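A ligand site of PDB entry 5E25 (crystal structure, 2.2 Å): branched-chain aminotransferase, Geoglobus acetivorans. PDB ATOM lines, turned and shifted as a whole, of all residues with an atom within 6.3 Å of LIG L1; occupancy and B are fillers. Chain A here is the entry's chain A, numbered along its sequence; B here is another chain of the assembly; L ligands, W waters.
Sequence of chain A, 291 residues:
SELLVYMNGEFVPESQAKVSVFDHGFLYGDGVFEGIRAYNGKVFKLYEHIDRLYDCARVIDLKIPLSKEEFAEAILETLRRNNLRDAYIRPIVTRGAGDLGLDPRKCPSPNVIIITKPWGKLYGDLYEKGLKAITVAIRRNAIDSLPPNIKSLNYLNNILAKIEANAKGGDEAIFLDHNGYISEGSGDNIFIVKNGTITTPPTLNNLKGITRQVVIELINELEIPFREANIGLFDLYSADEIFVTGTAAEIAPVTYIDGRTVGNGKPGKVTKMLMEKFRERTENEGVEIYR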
ATOM      1  N   PHE A  33     -15.777  14.436 -35.105  1.00  0.00           N
ATOM      2  CA  PHE A  33     -14.904  15.585 -35.278  1.00  0.00           C
ATOM      3  C   PHE A  33     -13.635  15.388 -34.496  1.00  0.00           C
ATOM      4  O   PHE A  33     -13.509  14.387 -33.764  1.00  0.00           O
ATOM      5  CB  PHE A  33     -15.541  16.943 -34.888  1.00  0.00           C
ATOM      6  CG  PHE A  33     -15.651  17.171 -33.399  1.00  0.00           C
ATOM      7  CD1 PHE A  33     -16.765  16.654 -32.690  1.00  0.00           C
ATOM      8  CD2 PHE A  33     -14.684  17.910 -32.697  1.00  0.00           C
ATOM      9  CE1 PHE A  33     -16.905  16.899 -31.304  1.00  0.00           C
ATOM     10  CE2 PHE A  33     -14.817  18.154 -31.317  1.00  0.00           C
ATOM     11  CZ  PHE A  33     -15.933  17.650 -30.628  1.00  0.00           C
ATOM     12  N   GLU A  34     -12.679  16.325 -34.721  1.00  0.00           N
ATOM     13  CA  GLU A  34     -11.412  16.335 -34.057  1.00  0.00           C
ATOM     14  C   GLU A  34     -11.048  17.717 -33.734  1.00  0.00           C
ATOM     15  O   GLU A  34     -11.680  18.653 -34.227  1.00  0.00           O
ATOM     16  CB  GLU A  34     -10.278  15.687 -34.871  1.00  0.00           C
ATOM     17  CG  GLU A  34     -10.209  14.206 -34.677  1.00  0.00           C
ATOM     18  CD  GLU A  34      -9.850  13.824 -33.266  1.00  0.00           C
ATOM     19  OE1 GLU A  34     -10.265  12.696 -32.877  1.00  0.00           O
ATOM     20  OE2 GLU A  34      -9.172  14.650 -32.548  1.00  0.00           O
ATOM     21  N   GLY A  35     -10.010  17.806 -32.883  1.00  0.00           N
ATOM     22  CA  GLY A  35      -9.449  19.085 -32.482  1.00  0.00           C
ATOM     23  C   GLY A  35      -7.941  18.892 -32.457  1.00  0.00           C
ATOM     24  O   GLY A  35      -7.463  17.971 -31.775  1.00  0.00           O
ATOM     25  N   ILE A  36      -7.221  19.715 -33.222  1.00  0.00           N
ATOM     26  CA  ILE A  36      -5.753  19.571 -33.477  1.00  0.00           C
ATOM     27  C   ILE A  36      -5.165  20.989 -33.439  1.00  0.00           C
ATOM     28  O   ILE A  36      -5.809  21.981 -33.870  1.00  0.00           O
ATOM     29  CB  ILE A  36      -5.431  18.842 -34.814  1.00  0.00           C
ATOM     30  CG1 ILE A  36      -6.425  17.705 -35.113  1.00  0.00           C
ATOM     31  CG2 ILE A  36      -4.027  18.219 -34.799  1.00  0.00           C
ATOM     32  CD1 ILE A  36      -6.301  16.989 -36.458  1.00  0.00           C
ATOM     33  N   TYR A  88      -5.708  26.305 -34.554  1.00  0.00           N
ATOM     34  CA  TYR A  88      -6.640  25.266 -34.192  1.00  0.00           C
ATOM     35  C   TYR A  88      -7.276  24.677 -35.441  1.00  0.00           C
ATOM     36  O   TYR A  88      -7.832  25.385 -36.295  1.00  0.00           O
ATOM     37  CB  TYR A  88      -7.751  25.826 -33.261  1.00  0.00           C
ATOM     38  CG  TYR A  88      -8.668  24.717 -32.746  1.00  0.00           C
ATOM     39  CD1 TYR A  88      -8.253  23.867 -31.701  1.00  0.00           C
ATOM     40  CD2 TYR A  88      -9.926  24.474 -33.346  1.00  0.00           C
ATOM     41  CE1 TYR A  88      -9.062  22.856 -31.221  1.00  0.00           C
ATOM     42  CE2 TYR A  88     -10.767  23.440 -32.886  1.00  0.00           C
ATOM     43  CZ  TYR A  88     -10.318  22.623 -31.819  1.00  0.00           C
ATOM     44  OH  TYR A  88     -11.103  21.596 -31.323  1.00  0.00           O
ATOM     45  N   ILE A  89      -7.237  23.353 -35.522  1.00  0.00           N
ATOM     46  CA  ILE A  89      -7.880  22.623 -36.605  1.00  0.00           C
ATOM     47  C   ILE A  89      -9.103  21.780 -36.097  1.00  0.00           C
ATOM     48  O   ILE A  89      -8.959  20.917 -35.164  1.00  0.00           O
ATOM     49  CB  ILE A  89      -6.899  21.711 -37.377  1.00  0.00           C
ATOM     50  CG1 ILE A  89      -5.618  22.451 -37.788  1.00  0.00           C
ATOM     51  CG2 ILE A  89      -7.583  21.042 -38.582  1.00  0.00           C
ATOM     52  CD1 ILE A  89      -4.347  21.936 -37.086  1.00  0.00           C
ATOM     53  N   ARG A  90     -10.258  22.004 -36.740  1.00  0.00           N
ATOM     54  CA  ARG A  90     -11.501  21.204 -36.581  1.00  0.00           C
ATOM     55  C   ARG A  90     -11.925  20.426 -37.835  1.00  0.00           C
ATOM     56  O   ARG A  90     -12.785  20.900 -38.598  1.00  0.00           O
ATOM     57  CB  ARG A  90     -12.637  22.157 -36.118  1.00  0.00           C
ATOM     58  CG  ARG A  90     -14.073  21.531 -35.958  1.00  0.00           C
ATOM     59  CD  ARG A  90     -14.149  20.353 -34.982  1.00  0.00           C
ATOM     60  NE  ARG A  90     -13.709  20.847 -33.680  1.00  0.00           N
ATOM     61  CZ  ARG A  90     -14.481  21.507 -32.784  1.00  0.00           C
ATOM     62  NH1 ARG A  90     -15.786  21.612 -32.964  1.00  0.00           N
ATOM     63  NH2 ARG A  90     -13.956  22.030 -31.684  1.00  0.00           N
ATOM     64  N   TRP A 119      -7.066  30.274 -32.652  1.00  0.00           N
ATOM     65  CA  TRP A 119      -8.055  30.171 -31.539  1.00  0.00           C
ATOM     66  C   TRP A 119      -7.248  30.003 -30.246  1.00  0.00           C
ATOM     67  O   TRP A 119      -6.576  28.950 -30.046  1.00  0.00           O
ATOM     68  CB  TRP A 119      -9.097  29.022 -31.751  1.00  0.00           C
ATOM     69  CG  TRP A 119     -10.237  28.888 -30.695  1.00  0.00           C
ATOM     70  CD1 TRP A 119     -10.914  29.920 -30.068  1.00  0.00           C
ATOM     71  CD2 TRP A 119     -10.833  27.667 -30.201  1.00  0.00           C
ATOM     72  NE1 TRP A 119     -11.865  29.399 -29.203  1.00  0.00           N
ATOM     73  CE2 TRP A 119     -11.843  28.026 -29.269  1.00  0.00           C
ATOM     74  CE3 TRP A 119     -10.619  26.292 -30.445  1.00  0.00           C
ATOM     75  CZ2 TRP A 119     -12.622  27.068 -28.580  1.00  0.00           C
ATOM     76  CZ3 TRP A 119     -11.410  25.338 -29.771  1.00  0.00           C
ATOM     77  CH2 TRP A 119     -12.378  25.731 -28.838  1.00  0.00           C
ATOM     78  N   LEU A 122      -8.196  27.495 -24.599  1.00  0.00           N
ATOM     79  CA  LEU A 122      -9.606  27.579 -24.170  1.00  0.00           C
ATOM     80  C   LEU A 122      -9.830  28.565 -22.991  1.00  0.00           C
ATOM     81  O   LEU A 122     -10.729  29.428 -23.072  1.00  0.00           O
ATOM     82  CB  LEU A 122     -10.183  26.192 -23.861  1.00  0.00           C
ATOM     83  CG  LEU A 122     -11.696  26.021 -23.634  1.00  0.00           C
ATOM     84  CD1 LEU A 122     -12.596  26.466 -24.812  1.00  0.00           C
ATOM     85  CD2 LEU A 122     -11.949  24.568 -23.220  1.00  0.00           C
ATOM     86  N   LYS A 151     -15.912  11.068 -30.266  1.00  0.00           N
ATOM     87  CA  LYS A 151     -15.870  12.547 -30.418  1.00  0.00           C
ATOM     88  C   LYS A 151     -16.815  12.851 -31.544  1.00  0.00           C
ATOM     89  O   LYS A 151     -16.406  12.905 -32.719  1.00  0.00           O
ATOM     90  CB  LYS A 151     -14.473  13.021 -30.804  1.00  0.00           C
ATOM     91  CG  LYS A 151     -14.128  14.352 -30.181  1.00  0.00           C
ATOM     92  CD  LYS A 151     -12.618  14.452 -30.229  1.00  0.00           C
ATOM     93  CE  LYS A 151     -12.329  15.883 -29.861  1.00  0.00           C
ATOM     94  NZ  LYS A 151     -12.558  16.130 -28.457  1.00  0.00           N
ATOM     95  N   TYR A 155     -23.072  16.636 -28.910  1.00  0.00           N
ATOM     96  CA  TYR A 155     -22.411  17.190 -27.740  1.00  0.00           C
ATOM     97  C   TYR A 155     -23.331  17.940 -26.797  1.00  0.00           C
ATOM     98  O   TYR A 155     -22.877  18.767 -26.021  1.00  0.00           O
ATOM     99  CB  TYR A 155     -21.148  18.035 -28.151  1.00  0.00           C
ATOM    100  CG  TYR A 155     -19.851  17.229 -27.980  1.00  0.00           C
ATOM    101  CD1 TYR A 155     -19.792  15.914 -28.437  1.00  0.00           C
ATOM    102  CD2 TYR A 155     -18.728  17.772 -27.305  1.00  0.00           C
ATOM    103  CE1 TYR A 155     -18.643  15.140 -28.245  1.00  0.00           C
ATOM    104  CE2 TYR A 155     -17.573  17.029 -27.124  1.00  0.00           C
ATOM    105  CZ  TYR A 155     -17.563  15.705 -27.610  1.00  0.00           C
ATOM    106  OH  TYR A 155     -16.486  14.907 -27.458  1.00  0.00           O
ATOM    107  N   SER A 186     -16.243  19.073 -19.167  1.00  0.00           N
ATOM    108  CA  SER A 186     -17.197  19.066 -20.323  1.00  0.00           C
ATOM    109  C   SER A 186     -16.498  18.843 -21.638  1.00  0.00           C
ATOM    110  O   SER A 186     -17.104  18.349 -22.602  1.00  0.00           O
ATOM    111  CB  SER A 186     -17.956  20.378 -20.431  1.00  0.00           C
ATOM    112  OG  SER A 186     -17.050  21.481 -20.511  1.00  0.00           O
ATOM    113  N   GLY A 187     -15.232  19.262 -21.701  1.00  0.00           N
ATOM    114  CA  GLY A 187     -14.425  19.181 -22.897  1.00  0.00           C
ATOM    115  C   GLY A 187     -12.961  18.811 -22.687  1.00  0.00           C
ATOM    116  O   GLY A 187     -12.135  18.953 -23.624  1.00  0.00           O
ATOM    117  N   ASP A 188     -12.637  18.347 -21.488  1.00  0.00           N
ATOM    118  CA  ASP A 188     -11.249  17.952 -21.211  1.00  0.00           C
ATOM    119  C   ASP A 188     -11.131  16.864 -20.145  1.00  0.00           C
ATOM    120  O   ASP A 188     -12.030  16.686 -19.327  1.00  0.00           O
ATOM    121  CB  ASP A 188     -10.407  19.191 -20.871  1.00  0.00           C
ATOM    122  CG  ASP A 188     -11.200  20.271 -20.232  1.00  0.00           C
ATOM    123  OD1 ASP A 188     -12.060  19.979 -19.356  1.00  0.00           O
ATOM    124  OD2 ASP A 188     -10.954  21.434 -20.596  1.00  0.00           O
ATOM    125  N   THR A 211      -4.156  14.651 -25.393  1.00  0.00           N
ATOM    126  CA  THR A 211      -3.349  15.418 -24.429  1.00  0.00           C
ATOM    127  C   THR A 211      -3.063  14.594 -23.146  1.00  0.00           C
ATOM    128  O   THR A 211      -1.961  14.632 -22.578  1.00  0.00           O
ATOM    129  CB  THR A 211      -4.020  16.719 -24.026  1.00  0.00           C
ATOM    130  OG1 THR A 211      -4.535  17.344 -25.191  1.00  0.00           O
ATOM    131  CG2 THR A 211      -3.018  17.664 -23.301  1.00  0.00           C
ATOM    132  N   GLY A 246      -6.730  18.971 -22.542  1.00  0.00           N
ATOM    133  CA  GLY A 246      -7.298  18.789 -23.888  1.00  0.00           C
ATOM    134  C   GLY A 246      -6.541  19.608 -24.943  1.00  0.00           C
ATOM    135  O   GLY A 246      -5.712  20.460 -24.584  1.00  0.00           O
ATOM    136  N   THR A 247      -6.820  19.381 -26.229  1.00  0.00           N
ATOM    137  CA  THR A 247      -6.101  20.097 -27.305  1.00  0.00           C
ATOM    138  C   THR A 247      -6.260  21.596 -27.165  1.00  0.00           C
ATOM    139  O   THR A 247      -5.271  22.304 -27.121  1.00  0.00           O
ATOM    140  CB  THR A 247      -6.443  19.608 -28.708  1.00  0.00           C
ATOM    141  OG1 THR A 247      -6.114  18.214 -28.775  1.00  0.00           O
ATOM    142  CG2 THR A 247      -5.618  20.420 -29.805  1.00  0.00           C
ATOM    143  N   ALA A 248      -7.484  22.054 -26.973  1.00  0.00           N
ATOM    144  CA  ALA A 248      -7.741  23.469 -26.931  1.00  0.00           C
ATOM    145  C   ALA A 248      -7.217  24.031 -25.627  1.00  0.00           C
ATOM    146  O   ALA A 248      -6.515  25.055 -25.618  1.00  0.00           O
ATOM    147  CB  ALA A 248      -9.232  23.724 -27.084  1.00  0.00           C
ATOM    148  N   ALA A 249      -7.508  23.334 -24.533  1.00  0.00           N
ATOM    149  CA  ALA A 249      -7.184  23.844 -23.201  1.00  0.00           C
ATOM    150  C   ALA A 249      -5.703  23.681 -22.862  1.00  0.00           C
ATOM    151  O   ALA A 249      -5.191  24.332 -21.967  1.00  0.00           O
ATOM    152  CB  ALA A 249      -8.049  23.145 -22.148  1.00  0.00           C
ATOM    153  N   TYR B  28     -22.360  20.515 -32.886  1.00  0.00           N
ATOM    154  CA  TYR B  28     -22.637  19.855 -31.600  1.00  0.00           C
ATOM    155  C   TYR B  28     -24.072  19.337 -31.402  1.00  0.00           C
ATOM    156  O   TYR B  28     -24.453  18.968 -30.274  1.00  0.00           O
ATOM    157  CB  TYR B  28     -22.361  20.871 -30.521  1.00  0.00           C
ATOM    158  CG  TYR B  28     -20.940  21.350 -30.445  1.00  0.00           C
ATOM    159  CD1 TYR B  28     -19.909  20.432 -30.339  1.00  0.00           C
ATOM    160  CD2 TYR B  28     -20.639  22.734 -30.410  1.00  0.00           C
ATOM    161  CE1 TYR B  28     -18.619  20.856 -30.213  1.00  0.00           C
ATOM    162  CE2 TYR B  28     -19.315  23.175 -30.306  1.00  0.00           C
ATOM    163  CZ  TYR B  28     -18.326  22.223 -30.201  1.00  0.00           C
ATOM    164  OH  TYR B  28     -17.002  22.576 -30.041  1.00  0.00           O
ATOM    165  N   LEU B 100     -15.587  28.155 -31.671  1.00  0.00           N
ATOM    166  CA  LEU B 100     -15.475  26.697 -31.842  1.00  0.00           C
ATOM    167  C   LEU B 100     -15.672  25.831 -30.565  1.00  0.00           C
ATOM    168  O   LEU B 100     -15.828  24.596 -30.691  1.00  0.00           O
ATOM    169  CB  LEU B 100     -14.185  26.288 -32.565  1.00  0.00           C
ATOM    170  CG  LEU B 100     -14.185  26.700 -34.044  1.00  0.00           C
ATOM    171  CD1 LEU B 100     -12.792  26.594 -34.619  1.00  0.00           C
ATOM    172  CD2 LEU B 100     -15.116  25.799 -34.813  1.00  0.00           C
ATOM    173  N   GLY B 101     -15.669  26.463 -29.390  1.00  0.00           N
ATOM    174  CA  GLY B 101     -15.889  25.754 -28.109  1.00  0.00           C
ATOM    175  C   GLY B 101     -17.378  25.520 -27.813  1.00  0.00           C
ATOM    176  O   GLY B 101     -18.251  25.982 -28.543  1.00  0.00           O
ATOM    177  N   LEU B 102     -17.648  24.828 -26.708  1.00  0.00           N
ATOM    178  CA  LEU B 102     -18.982  24.410 -26.281  1.00  0.00           C
ATOM    179  C   LEU B 102     -19.904  25.534 -25.840  1.00  0.00           C
ATOM    180  O   LEU B 102     -21.123  25.363 -25.870  1.00  0.00           O
ATOM    181  CB  LEU B 102     -18.827  23.461 -25.055  1.00  0.00           C
ATOM    182  CG  LEU B 102     -18.762  21.961 -25.328  1.00  0.00           C
ATOM    183  CD1 LEU B 102     -18.680  21.664 -26.797  1.00  0.00           C
ATOM    184  CD2 LEU B 102     -17.676  21.189 -24.607  1.00  0.00           C
HETATM  185  C1  LIG L   1     -10.376  20.118 -28.151  1.00  0.00           C
HETATM  186  O1  LIG L   1      -9.913  20.521 -29.244  1.00  0.00           O
HETATM  187  O2  LIG L   1      -9.704  20.070 -27.085  1.00  0.00           O
HETATM  188  C2  LIG L   1     -11.785  19.693 -28.184  1.00  0.00           C
HETATM  189  O3  LIG L   1     -12.238  19.477 -29.304  1.00  0.00           O
HETATM  190  C3  LIG L   1     -12.632  19.589 -26.910  1.00  0.00           C
HETATM  191  C4  LIG L   1     -14.143  19.660 -27.118  1.00  0.00           C
HETATM  192  C5  LIG L   1     -14.679  20.913 -27.855  1.00  0.00           C
HETATM  193  O4  LIG L   1     -15.778  20.771 -28.411  1.00  0.00           O
HETATM  194  O5  LIG L   1     -14.071  22.022 -27.907  1.00  0.00           O
HETATM  195  N1  LG2 L   2     -12.987  15.274 -23.488  1.00  0.00           N
HETATM  196  C1  LG2 L   2     -13.932  15.487 -24.429  1.00  0.00           C
HETATM  197  C2  LG2 L   2     -15.399  15.325 -24.081  1.00  0.00           C
HETATM  198  C3  LG2 L   2     -13.522  15.870 -25.810  1.00  0.00           C
HETATM  199  O1  LG2 L   2     -14.459  16.073 -26.772  1.00  0.00           O
HETATM  200  C4  LG2 L   2     -12.059  16.014 -26.082  1.00  0.00           C
HETATM  201  C5  LG2 L   2     -11.528  16.369 -27.486  1.00  0.00           C
HETATM  202  C6  LG2 L   2     -11.159  15.804 -24.910  1.00  0.00           C
HETATM  203  C7  LG2 L   2     -11.681  15.403 -23.666  1.00  0.00           C
HETATM  204  C8  LG2 L   2      -9.665  15.961 -24.984  1.00  0.00           C
HETATM  205  O2  LG2 L   2      -9.120  15.216 -26.058  1.00  0.00           O
HETATM  206  P1  LG2 L   2      -7.665  15.660 -26.626  1.00  0.00           P
HETATM  207  O3  LG2 L   2      -7.957  17.058 -27.105  1.00  0.00           O
HETATM  208  O4  LG2 L   2      -6.744  15.805 -25.476  1.00  0.00           O
HETATM  209  O5  LG2 L   2      -7.490  14.526 -27.596  1.00  0.00           O
HETATM  210  O   HOH W   1      -9.565  21.182 -24.490  1.00  0.00           O
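NH2 of Arg 90 is in hydrogen-bond range of OH of Tyr 88 (2.9 Å).
The side-chain hydroxyl of Tyr 28 of chain B lies within hydrogen-bond range of the guanidinium group of Arg 90, at 3.3 Å.
The backbone carbonyl oxygen of Leu 100 of chain B lies within hydrogen-bond range of the side-chain hydroxyl of Tyr 28 of chain B, 2.4 Å away.
N of Tyr 155 is in hydrogen-bond range of O of Tyr 28 of chain B.
N of Leu 122 sits at hydrogen-bond distance from O of Ala 248 (3.1 Å).
OG1 of Thr 247 lies within hydrogen-bond range of O of Gly 35, at 3.3 Å.
The backbone carbonyl oxygen of Lys 151 is in hydrogen-bond range of the backbone NH of Phe 33, 2.9 Å away.
O of Gly 246 lies close to OG1 of Thr 211, at 3.4 Å.
Water W1 lies within hydrogen-bond range of O2 of LIG L1, N of Ala 249 and N of Ala 248.
CE2 of Phe 33 touches O3 of LIG L1, at 3.5 Å.
Gly 35 touches LIG L1.
Gly 187 touches LIG L1.
C of Gly 246 touches O2 of LIG L1 (3.8 Å).
CD1 of Leu 102 of chain B touches O4 of LIG L1 (3.4 Å).
Hydrophobic or aromatic side chains within 4 Å of LIG L1: Phe 33, Tyr 88, Ala 248, Tyr 28 of chain B and Leu 102 of chain B.
Of the 23 residues printed, 11 come within 4 Å of LIG L1.
The side-chain hydroxyl (OH) of Tyr 88 is in hydrogen-bond range of an oxygen (O1) of LIG L1.
The side-chain hydroxyl (OH) of Tyr 28 of chain B lies within hydrogen-bond range of an oxygen (O4) of LIG L1 (2.7 Å).
The backbone NH (N) of Ala 248 lies within hydrogen-bond range of an oxygen (O2) of LIG L1 (3.0 Å).
The backbone NH (N) of Thr 247 sits at hydrogen-bond distance from an oxygen (O2) of LIG L1, at 3.1 Å.
An oxygen (O3) of LIG L1 is in hydrogen-bond range of the side-chain amino group (NZ) of Lys 151.
The guanidinium group (NH2) of Arg 90 lies within salt-bridge range of an oxygen (O5) of LIG L1 (3.8 Å).
The backbone NH (N) of Thr 247 sits at hydrogen-bond distance from an oxygen (O3) of LG2 L2.
OG1 of Thr 247 sits at hydrogen-bond distance from O3 of LG2 L2 (2.7 Å).
The side-chain amino group of Lys 151 is bonded to a carbon (C5) of LG2 L2, at 1.4 Å.
The side-chain hydroxyl (OH) of Tyr 155 is in hydrogen-bond range of an oxygen (O1) of LG2 L2 (2.4 Å).
The backbone NH (N) of Thr 211 lies within hydrogen-bond range of an oxygen (O4) of LG2 L2 (2.8 Å).
The side-chain hydroxyl (OG1) of Thr 211 sits at hydrogen-bond distance from an oxygen (O4) of LG2 L2 (2.7 Å).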
